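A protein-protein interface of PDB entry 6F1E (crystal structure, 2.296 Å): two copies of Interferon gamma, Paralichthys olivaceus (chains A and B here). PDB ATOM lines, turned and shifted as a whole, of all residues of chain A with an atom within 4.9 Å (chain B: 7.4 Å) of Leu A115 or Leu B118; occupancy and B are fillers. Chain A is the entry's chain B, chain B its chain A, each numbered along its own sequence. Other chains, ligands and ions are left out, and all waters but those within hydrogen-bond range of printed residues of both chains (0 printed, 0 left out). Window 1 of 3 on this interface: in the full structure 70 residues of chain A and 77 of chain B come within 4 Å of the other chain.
The backbone carbonyl oxygen of Leu B115 sits at hydrogen-bond distance from a ring nitrogen (ND1) of His B119.
The backbone carbonyl oxygen of Leu A115 sits close to a ring nitrogen (ND1) of His A119, 3.4 Å away.
Leu B46 touches Leu A46.
Gly A50 touches Leu B121 (C to CD1, 3.6 Å).
Leu A115 touches Leu B118.
CD2 of Leu A118 touches CD2 of Leu B115, 3.6 Å away.
Of the printed residues of chain B, Leu A115 touches Leu B118 (3.8 Å).
Leu B118 touches just one residue of chain A: Leu A115 (3.8 Å).
Of the printed residues of chain B, Leu A46 touches Leu B46 (3.2 Å).
Of the printed residues of chain B, Gly A50 touches Leu B121.
Of the printed residues of chain A, Leu B46 touches Leu A46.
Gln B111 touches none of the printed residues of chain A.
The nearest residue of chain B that does not touch Leu A115 is Leu B121 (6.5 Å).
The nearest residue of chain A that does not touch Leu B118 is Leu A118 (4.1 Å).
The nearest printed residue of chain A that does not touch Leu B46 is Leu A118 (4.2 Å).
Hydrophobic or aromatic side chains of chain B within 4 Å of the printed part of chain A: Leu B46, Leu B115, Leu B118 and Leu B121.
Among the printed residues, 4 pairs touch across the chains.
Leu A46 touches its own counterpart, Leu B46.
Leu A115 touches Leu B118, and with the chains exchanged Leu A118 touches Leu B115.
Positions printed for both chains: 46, 111, 112, 113, 114, 115, 116, 117, 118 and 119.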
ATOM      1  N   LEU A  46       4.465  19.652 -24.416  1.00  0.00           N
ATOM      2  CA  LEU A  46       3.058  19.609 -24.121  1.00  0.00           C
ATOM      3  C   LEU A  46       2.670  18.345 -23.354  1.00  0.00           C
ATOM      4  O   LEU A  46       1.924  18.382 -22.368  1.00  0.00           O
ATOM      5  CB  LEU A  46       2.292  19.677 -25.449  1.00  0.00           C
ATOM      6  CG  LEU A  46       0.831  20.058 -25.413  1.00  0.00           C
ATOM      7  CD1 LEU A  46       0.587  21.396 -24.717  1.00  0.00           C
ATOM      8  CD2 LEU A  46       0.384  20.138 -26.855  1.00  0.00           C
ATOM      9  N   PHE A  47       3.191  17.217 -23.815  1.00  0.00           N
ATOM     10  CA  PHE A  47       2.929  15.968 -23.145  1.00  0.00           C
ATOM     11  C   PHE A  47       3.428  16.112 -21.717  1.00  0.00           C
ATOM     12  O   PHE A  47       2.686  15.864 -20.777  1.00  0.00           O
ATOM     13  CB  PHE A  47       3.595  14.813 -23.873  1.00  0.00           C
ATOM     14  CG  PHE A  47       3.368  13.485 -23.230  1.00  0.00           C
ATOM     15  CD1 PHE A  47       2.196  12.795 -23.425  1.00  0.00           C
ATOM     16  CD2 PHE A  47       4.340  12.918 -22.456  1.00  0.00           C
ATOM     17  CE1 PHE A  47       1.985  11.563 -22.843  1.00  0.00           C
ATOM     18  CE2 PHE A  47       4.146  11.683 -21.856  1.00  0.00           C
ATOM     19  CZ  PHE A  47       2.970  11.002 -22.060  1.00  0.00           C
ATOM     20  N   GLY A  49       3.963  18.759 -19.950  1.00  0.00           N
ATOM     21  CA  GLY A  49       3.029  19.670 -19.263  1.00  0.00           C
ATOM     22  C   GLY A  49       1.807  18.912 -18.758  1.00  0.00           C
ATOM     23  O   GLY A  49       1.327  19.150 -17.654  1.00  0.00           O
ATOM     24  N   GLY A  50       1.291  18.005 -19.586  1.00  0.00           N
ATOM     25  CA  GLY A  50       0.261  17.074 -19.167  1.00  0.00           C
ATOM     26  C   GLY A  50       0.747  16.293 -17.972  1.00  0.00           C
ATOM     27  O   GLY A  50       0.023  16.078 -16.996  1.00  0.00           O
ATOM     28  N   GLU A  53       0.992  18.374 -14.591  1.00  0.00           N
ATOM     29  CA  GLU A  53      -0.358  18.670 -14.184  1.00  0.00           C
ATOM     30  C   GLU A  53      -0.955  17.478 -13.485  1.00  0.00           C
ATOM     31  O   GLU A  53      -1.480  17.604 -12.371  1.00  0.00           O
ATOM     32  CB  GLU A  53      -1.183  19.033 -15.381  1.00  0.00           C
ATOM     33  CG  GLU A  53      -2.632  19.364 -15.070  1.00  0.00           C
ATOM     34  CD  GLU A  53      -3.347  19.837 -16.322  1.00  0.00           C
ATOM     35  OE1 GLU A  53      -3.937  18.970 -17.001  1.00  0.00           O
ATOM     36  OE2 GLU A  53      -3.240  21.041 -16.657  1.00  0.00           O
ATOM     37  N   GLN A 111       2.033  25.771 -22.614  1.00  0.00           N
ATOM     38  CA  GLN A 111       1.510  24.420 -22.728  1.00  0.00           C
ATOM     39  C   GLN A 111       0.253  24.294 -21.876  1.00  0.00           C
ATOM     40  O   GLN A 111      -0.727  23.693 -22.309  1.00  0.00           O
ATOM     41  CB  GLN A 111       2.568  23.403 -22.317  1.00  0.00           C
ATOM     42  CG  GLN A 111       3.697  23.244 -23.330  1.00  0.00           C
ATOM     43  CD  GLN A 111       4.666  24.405 -23.426  1.00  0.00           C
ATOM     44  OE1 GLN A 111       4.542  25.398 -22.718  1.00  0.00           O
ATOM     45  NE2 GLN A 111       5.652  24.274 -24.309  1.00  0.00           N
ATOM     46  N   SER A 112       0.294  24.903 -20.692  1.00  0.00           N
ATOM     47  CA  SER A 112      -0.838  24.923 -19.758  1.00  0.00           C
ATOM     48  C   SER A 112      -2.082  25.674 -20.294  1.00  0.00           C
ATOM     49  O   SER A 112      -3.203  25.212 -20.121  1.00  0.00           O
ATOM     50  CB  SER A 112      -0.385  25.477 -18.389  1.00  0.00           C
ATOM     51  OG  SER A 112       0.566  24.608 -17.734  1.00  0.00           O
ATOM     52  N   LYS A 113      -1.896  26.807 -20.959  1.00  0.00           N
ATOM     53  CA  LYS A 113      -3.022  27.500 -21.598  1.00  0.00           C
ATOM     54  C   LYS A 113      -3.719  26.626 -22.686  1.00  0.00           C
ATOM     55  O   LYS A 113      -4.965  26.660 -22.845  1.00  0.00           O
ATOM     56  CB  LYS A 113      -2.561  28.870 -22.146  1.00  0.00           C
ATOM     57  CG  LYS A 113      -3.545  29.614 -23.064  1.00  0.00           C
ATOM     58  CD  LYS A 113      -3.443  31.151 -23.032  1.00  0.00           C
ATOM     59  CE  LYS A 113      -2.019  31.718 -22.993  1.00  0.00           C
ATOM     60  NZ  LYS A 113      -1.112  31.270 -24.097  1.00  0.00           N
ATOM     61  N   LEU A 114      -2.927  25.831 -23.407  1.00  0.00           N
ATOM     62  CA  LEU A 114      -3.469  24.915 -24.434  1.00  0.00           C
ATOM     63  C   LEU A 114      -4.171  23.684 -23.839  1.00  0.00           C
ATOM     64  O   LEU A 114      -5.223  23.259 -24.304  1.00  0.00           O
ATOM     65  CB  LEU A 114      -2.343  24.460 -25.352  1.00  0.00           C
ATOM     66  CG  LEU A 114      -2.780  23.655 -26.568  1.00  0.00           C
ATOM     67  CD1 LEU A 114      -3.838  24.409 -27.350  1.00  0.00           C
ATOM     68  CD2 LEU A 114      -1.575  23.336 -27.449  1.00  0.00           C
ATOM     69  N   LEU A 115      -3.567  23.113 -22.808  1.00  0.00           N
ATOM     70  CA  LEU A 115      -4.122  21.962 -22.123  1.00  0.00           C
ATOM     71  C   LEU A 115      -5.478  22.268 -21.536  1.00  0.00           C
ATOM     72  O   LEU A 115      -6.374  21.399 -21.567  1.00  0.00           O
ATOM     73  CB  LEU A 115      -3.161  21.468 -21.038  1.00  0.00           C
ATOM     74  CG  LEU A 115      -1.938  20.751 -21.629  1.00  0.00           C
ATOM     75  CD1 LEU A 115      -0.723  20.795 -20.719  1.00  0.00           C
ATOM     76  CD2 LEU A 115      -2.308  19.319 -21.933  1.00  0.00           C
ATOM     77  N   GLN A 116      -5.633  23.502 -21.038  1.00  0.00           N
ATOM     78  CA  GLN A 116      -6.916  23.984 -20.463  1.00  0.00           C
ATOM     79  C   GLN A 116      -7.976  24.051 -21.571  1.00  0.00           C
ATOM     80  O   GLN A 116      -9.079  23.489 -21.431  1.00  0.00           O
ATOM     81  CB  GLN A 116      -6.733  25.348 -19.727  1.00  0.00           C
ATOM     82  CG  GLN A 116      -7.734  25.685 -18.586  1.00  0.00           C
ATOM     83  CD  GLN A 116      -8.251  24.494 -17.732  1.00  0.00           C
ATOM     84  OE1 GLN A 116      -9.457  24.259 -17.648  1.00  0.00           O
ATOM     85  NE2 GLN A 116      -7.348  23.747 -17.118  1.00  0.00           N
ATOM     86  N   GLY A 117      -7.626  24.688 -22.696  1.00  0.00           N
ATOM     87  CA  GLY A 117      -8.449  24.603 -23.920  1.00  0.00           C
ATOM     88  C   GLY A 117      -8.880  23.162 -24.224  1.00  0.00           C
ATOM     89  O   GLY A 117     -10.063  22.857 -24.452  1.00  0.00           O
ATOM     90  N   LEU A 118      -7.919  22.252 -24.193  1.00  0.00           N
ATOM     91  CA  LEU A 118      -8.227  20.889 -24.529  1.00  0.00           C
ATOM     92  C   LEU A 118      -9.136  20.280 -23.479  1.00  0.00           C
ATOM     93  O   LEU A 118     -10.034  19.511 -23.825  1.00  0.00           O
ATOM     94  CB  LEU A 118      -6.943  20.084 -24.818  1.00  0.00           C
ATOM     95  CG  LEU A 118      -6.245  20.602 -26.097  1.00  0.00           C
ATOM     96  CD1 LEU A 118      -4.779  20.218 -26.240  1.00  0.00           C
ATOM     97  CD2 LEU A 118      -7.038  20.173 -27.333  1.00  0.00           C
ATOM     98  N   HIS A 119      -8.965  20.645 -22.211  1.00  0.00           N
ATOM     99  CA  HIS A 119      -9.875  20.114 -21.179  1.00  0.00           C
ATOM    100  C   HIS A 119     -11.269  20.726 -21.346  1.00  0.00           C
ATOM    101  O   HIS A 119     -12.284  20.043 -21.166  1.00  0.00           O
ATOM    102  CB  HIS A 119      -9.349  20.335 -19.750  1.00  0.00           C
ATOM    103  CG  HIS A 119      -7.978  19.771 -19.501  1.00  0.00           C
ATOM    104  ND1 HIS A 119      -7.530  18.600 -20.080  1.00  0.00           N
ATOM    105  CD2 HIS A 119      -6.960  20.216 -18.725  1.00  0.00           C
ATOM    106  CE1 HIS A 119      -6.297  18.351 -19.679  1.00  0.00           C
ATOM    107  NE2 HIS A 119      -5.926  19.322 -18.863  1.00  0.00           N
ATOM    108  N   LEU B  46      -3.502  21.137 -33.336  1.00  0.00           N
ATOM    109  CA  LEU B  46      -3.807  20.279 -32.203  1.00  0.00           C
ATOM    110  C   LEU B  46      -5.190  20.626 -31.647  1.00  0.00           C
ATOM    111  O   LEU B  46      -6.033  19.737 -31.361  1.00  0.00           O
ATOM    112  CB  LEU B  46      -2.721  20.447 -31.136  1.00  0.00           C
ATOM    113  CG  LEU B  46      -2.769  19.483 -29.951  1.00  0.00           C
ATOM    114  CD1 LEU B  46      -3.301  18.088 -30.249  1.00  0.00           C
ATOM    115  CD2 LEU B  46      -1.361  19.375 -29.418  1.00  0.00           C
ATOM    116  N   GLN B 111      -2.113  14.321 -34.541  1.00  0.00           N
ATOM    117  CA  GLN B 111      -2.761  15.113 -33.528  1.00  0.00           C
ATOM    118  C   GLN B 111      -3.680  14.238 -32.687  1.00  0.00           C
ATOM    119  O   GLN B 111      -3.713  14.372 -31.473  1.00  0.00           O
ATOM    120  CB  GLN B 111      -3.526  16.252 -34.147  1.00  0.00           C
ATOM    121  CG  GLN B 111      -2.655  17.360 -34.725  1.00  0.00           C
ATOM    122  CD  GLN B 111      -2.017  17.053 -36.075  1.00  0.00           C
ATOM    123  OE1 GLN B 111      -2.351  16.070 -36.741  1.00  0.00           O
ATOM    124  NE2 GLN B 111      -1.093  17.902 -36.484  1.00  0.00           N
ATOM    125  N   SER B 112      -4.433  13.351 -33.322  1.00  0.00           N
ATOM    126  CA  SER B 112      -5.268  12.397 -32.589  1.00  0.00           C
ATOM    127  C   SER B 112      -4.469  11.527 -31.608  1.00  0.00           C
ATOM    128  O   SER B 112      -4.988  11.149 -30.535  1.00  0.00           O
ATOM    129  CB  SER B 112      -6.011  11.469 -33.569  1.00  0.00           C
ATOM    130  OG  SER B 112      -7.130  12.110 -34.135  1.00  0.00           O
ATOM    131  N   LYS B 113      -3.231  11.208 -32.002  1.00  0.00           N
ATOM    132  CA  LYS B 113      -2.333  10.337 -31.237  1.00  0.00           C
ATOM    133  C   LYS B 113      -1.978  11.016 -29.922  1.00  0.00           C
ATOM    134  O   LYS B 113      -2.171  10.442 -28.835  1.00  0.00           O
ATOM    135  CB  LYS B 113      -1.046  10.055 -32.052  1.00  0.00           C
ATOM    136  CG  LYS B 113      -0.310   8.752 -31.737  1.00  0.00           C
ATOM    137  CD  LYS B 113       0.763   8.450 -32.802  1.00  0.00           C
ATOM    138  CE  LYS B 113       0.182   7.876 -34.109  1.00  0.00           C
ATOM    139  NZ  LYS B 113       0.852   8.371 -35.353  1.00  0.00           N
ATOM    140  N   LEU B 114      -1.495  12.256 -30.051  1.00  0.00           N
ATOM    141  CA  LEU B 114      -1.147  13.114 -28.917  1.00  0.00           C
ATOM    142  C   LEU B 114      -2.344  13.315 -28.044  1.00  0.00           C
ATOM    143  O   LEU B 114      -2.293  13.022 -26.861  1.00  0.00           O
ATOM    144  CB  LEU B 114      -0.596  14.485 -29.361  1.00  0.00           C
ATOM    145  CG  LEU B 114      -0.150  15.477 -28.261  1.00  0.00           C
ATOM    146  CD1 LEU B 114       0.591  14.851 -27.096  1.00  0.00           C
ATOM    147  CD2 LEU B 114       0.738  16.564 -28.850  1.00  0.00           C
ATOM    148  N   LEU B 115      -3.432  13.776 -28.639  1.00  0.00           N
ATOM    149  CA  LEU B 115      -4.666  13.954 -27.901  1.00  0.00           C
ATOM    150  C   LEU B 115      -5.055  12.702 -27.132  1.00  0.00           C
ATOM    151  O   LEU B 115      -5.530  12.842 -26.007  1.00  0.00           O
ATOM    152  CB  LEU B 115      -5.823  14.414 -28.806  1.00  0.00           C
ATOM    153  CG  LEU B 115      -5.740  15.866 -29.344  1.00  0.00           C
ATOM    154  CD1 LEU B 115      -6.937  16.156 -30.231  1.00  0.00           C
ATOM    155  CD2 LEU B 115      -5.651  16.950 -28.263  1.00  0.00           C
ATOM    156  N   GLN B 116      -4.848  11.491 -27.675  1.00  0.00           N
ATOM    157  CA  GLN B 116      -5.257  10.284 -26.909  1.00  0.00           C
ATOM    158  C   GLN B 116      -4.372  10.146 -25.653  1.00  0.00           C
ATOM    159  O   GLN B 116      -4.865   9.817 -24.577  1.00  0.00           O
ATOM    160  CB  GLN B 116      -5.286   8.992 -27.755  1.00  0.00           C
ATOM    161  CG  GLN B 116      -5.964   7.749 -27.101  1.00  0.00           C
ATOM    162  CD  GLN B 116      -7.410   7.984 -26.623  1.00  0.00           C
ATOM    163  OE1 GLN B 116      -8.271   8.439 -27.376  1.00  0.00           O
ATOM    164  NE2 GLN B 116      -7.674   7.668 -25.363  1.00  0.00           N
ATOM    165  N   GLY B 117      -3.084  10.450 -25.795  1.00  0.00           N
ATOM    166  CA  GLY B 117      -2.193  10.584 -24.643  1.00  0.00           C
ATOM    167  C   GLY B 117      -2.722  11.575 -23.597  1.00  0.00           C
ATOM    168  O   GLY B 117      -2.902  11.215 -22.410  1.00  0.00           O
ATOM    169  N   LEU B 118      -3.010  12.801 -24.039  1.00  0.00           N
ATOM    170  CA  LEU B 118      -3.508  13.819 -23.114  1.00  0.00           C
ATOM    171  C   LEU B 118      -4.813  13.391 -22.498  1.00  0.00           C
ATOM    172  O   LEU B 118      -5.026  13.629 -21.333  1.00  0.00           O
ATOM    173  CB  LEU B 118      -3.662  15.192 -23.750  1.00  0.00           C
ATOM    174  CG  LEU B 118      -2.349  15.709 -24.341  1.00  0.00           C
ATOM    175  CD1 LEU B 118      -2.500  17.106 -24.957  1.00  0.00           C
ATOM    176  CD2 LEU B 118      -1.255  15.697 -23.283  1.00  0.00           C
ATOM    177  N   HIS B 119      -5.665  12.717 -23.247  1.00  0.00           N
ATOM    178  CA  HIS B 119      -6.968  12.335 -22.700  1.00  0.00           C
ATOM    179  C   HIS B 119      -6.763  11.246 -21.669  1.00  0.00           C
ATOM    180  O   HIS B 119      -7.387  11.247 -20.598  1.00  0.00           O
ATOM    181  CB  HIS B 119      -7.945  11.925 -23.812  1.00  0.00           C
ATOM    182  CG  HIS B 119      -8.474  13.089 -24.608  1.00  0.00           C
ATOM    183  ND1 HIS B 119      -7.717  14.210 -24.896  1.00  0.00           N
ATOM    184  CD2 HIS B 119      -9.683  13.302 -25.181  1.00  0.00           C
ATOM    185  CE1 HIS B 119      -8.432  15.059 -25.611  1.00  0.00           C
ATOM    186  NE2 HIS B 119      -9.628  14.533 -25.798  1.00  0.00           N
ATOM    187  N   ASP B 120      -5.841  10.350 -21.983  1.00  0.00           N
ATOM    188  CA  ASP B 120      -5.465   9.280 -21.065  1.00  0.00           C
ATOM    189  C   ASP B 120      -4.915   9.770 -19.698  1.00  0.00           C
ATOM    190  O   ASP B 120      -5.376   9.301 -18.666  1.00  0.00           O
ATOM    191  CB  ASP B 120      -4.519   8.275 -21.767  1.00  0.00           C
ATOM    192  CG  ASP B 120      -5.273   7.344 -22.768  1.00  0.00           C
ATOM    193  OD1 ASP B 120      -6.545   7.271 -22.723  1.00  0.00           O
ATOM    194  OD2 ASP B 120      -4.575   6.690 -23.584  1.00  0.00           O
ATOM    195  N   LEU B 121      -3.968  10.705 -19.708  1.00  0.00           N
ATOM    196  CA  LEU B 121      -3.460  11.360 -18.499  1.00  0.00           C
ATOM    197  C   LEU B 121      -4.576  11.959 -17.678  1.00  0.00           C
ATOM    198  O   LEU B 121      -4.601  11.810 -16.454  1.00  0.00           O
ATOM    199  CB  LEU B 121      -2.530  12.506 -18.874  1.00  0.00           C
ATOM    200  CG  LEU B 121      -1.166  12.137 -19.416  1.00  0.00           C
ATOM    201  CD1 LEU B 121      -0.440  13.411 -19.824  1.00  0.00           C
ATOM    202  CD2 LEU B 121      -0.361  11.402 -18.369  1.00  0.00           C
ATOM    203  N   GLY B 122      -5.492  12.631 -18.371  1.00  0.00           N
ATOM    204  CA  GLY B 122      -6.703  13.194 -17.775  1.00  0.00           C
ATOM    205  C   GLY B 122      -7.593  12.207 -17.025  1.00  0.00           C
ATOM    206  O   GLY B 122      -8.342  12.591 -16.125  1.00  0.00           O
ATOM    207  N   ASP B 123      -7.497  10.938 -17.375  1.00  0.00           N
ATOM    208  CA  ASP B 123      -8.453   9.921 -16.946  1.00  0.00           C
ATOM    209  C   ASP B 123      -7.888   9.090 -15.863  1.00  0.00           C
ATOM    210  O   ASP B 123      -8.571   8.197 -15.375  1.00  0.00           O
ATOM    211  CB  ASP B 123      -8.799   8.976 -18.126  1.00  0.00           C
ATOM    212  CG  ASP B 123      -9.893   9.526 -19.036  1.00  0.00           C
ATOM    213  OD1 ASP B 123     -10.269  10.737 -18.961  1.00  0.00           O
ATOM    214  OD2 ASP B 123     -10.384   8.698 -19.835  1.00  0.00           O
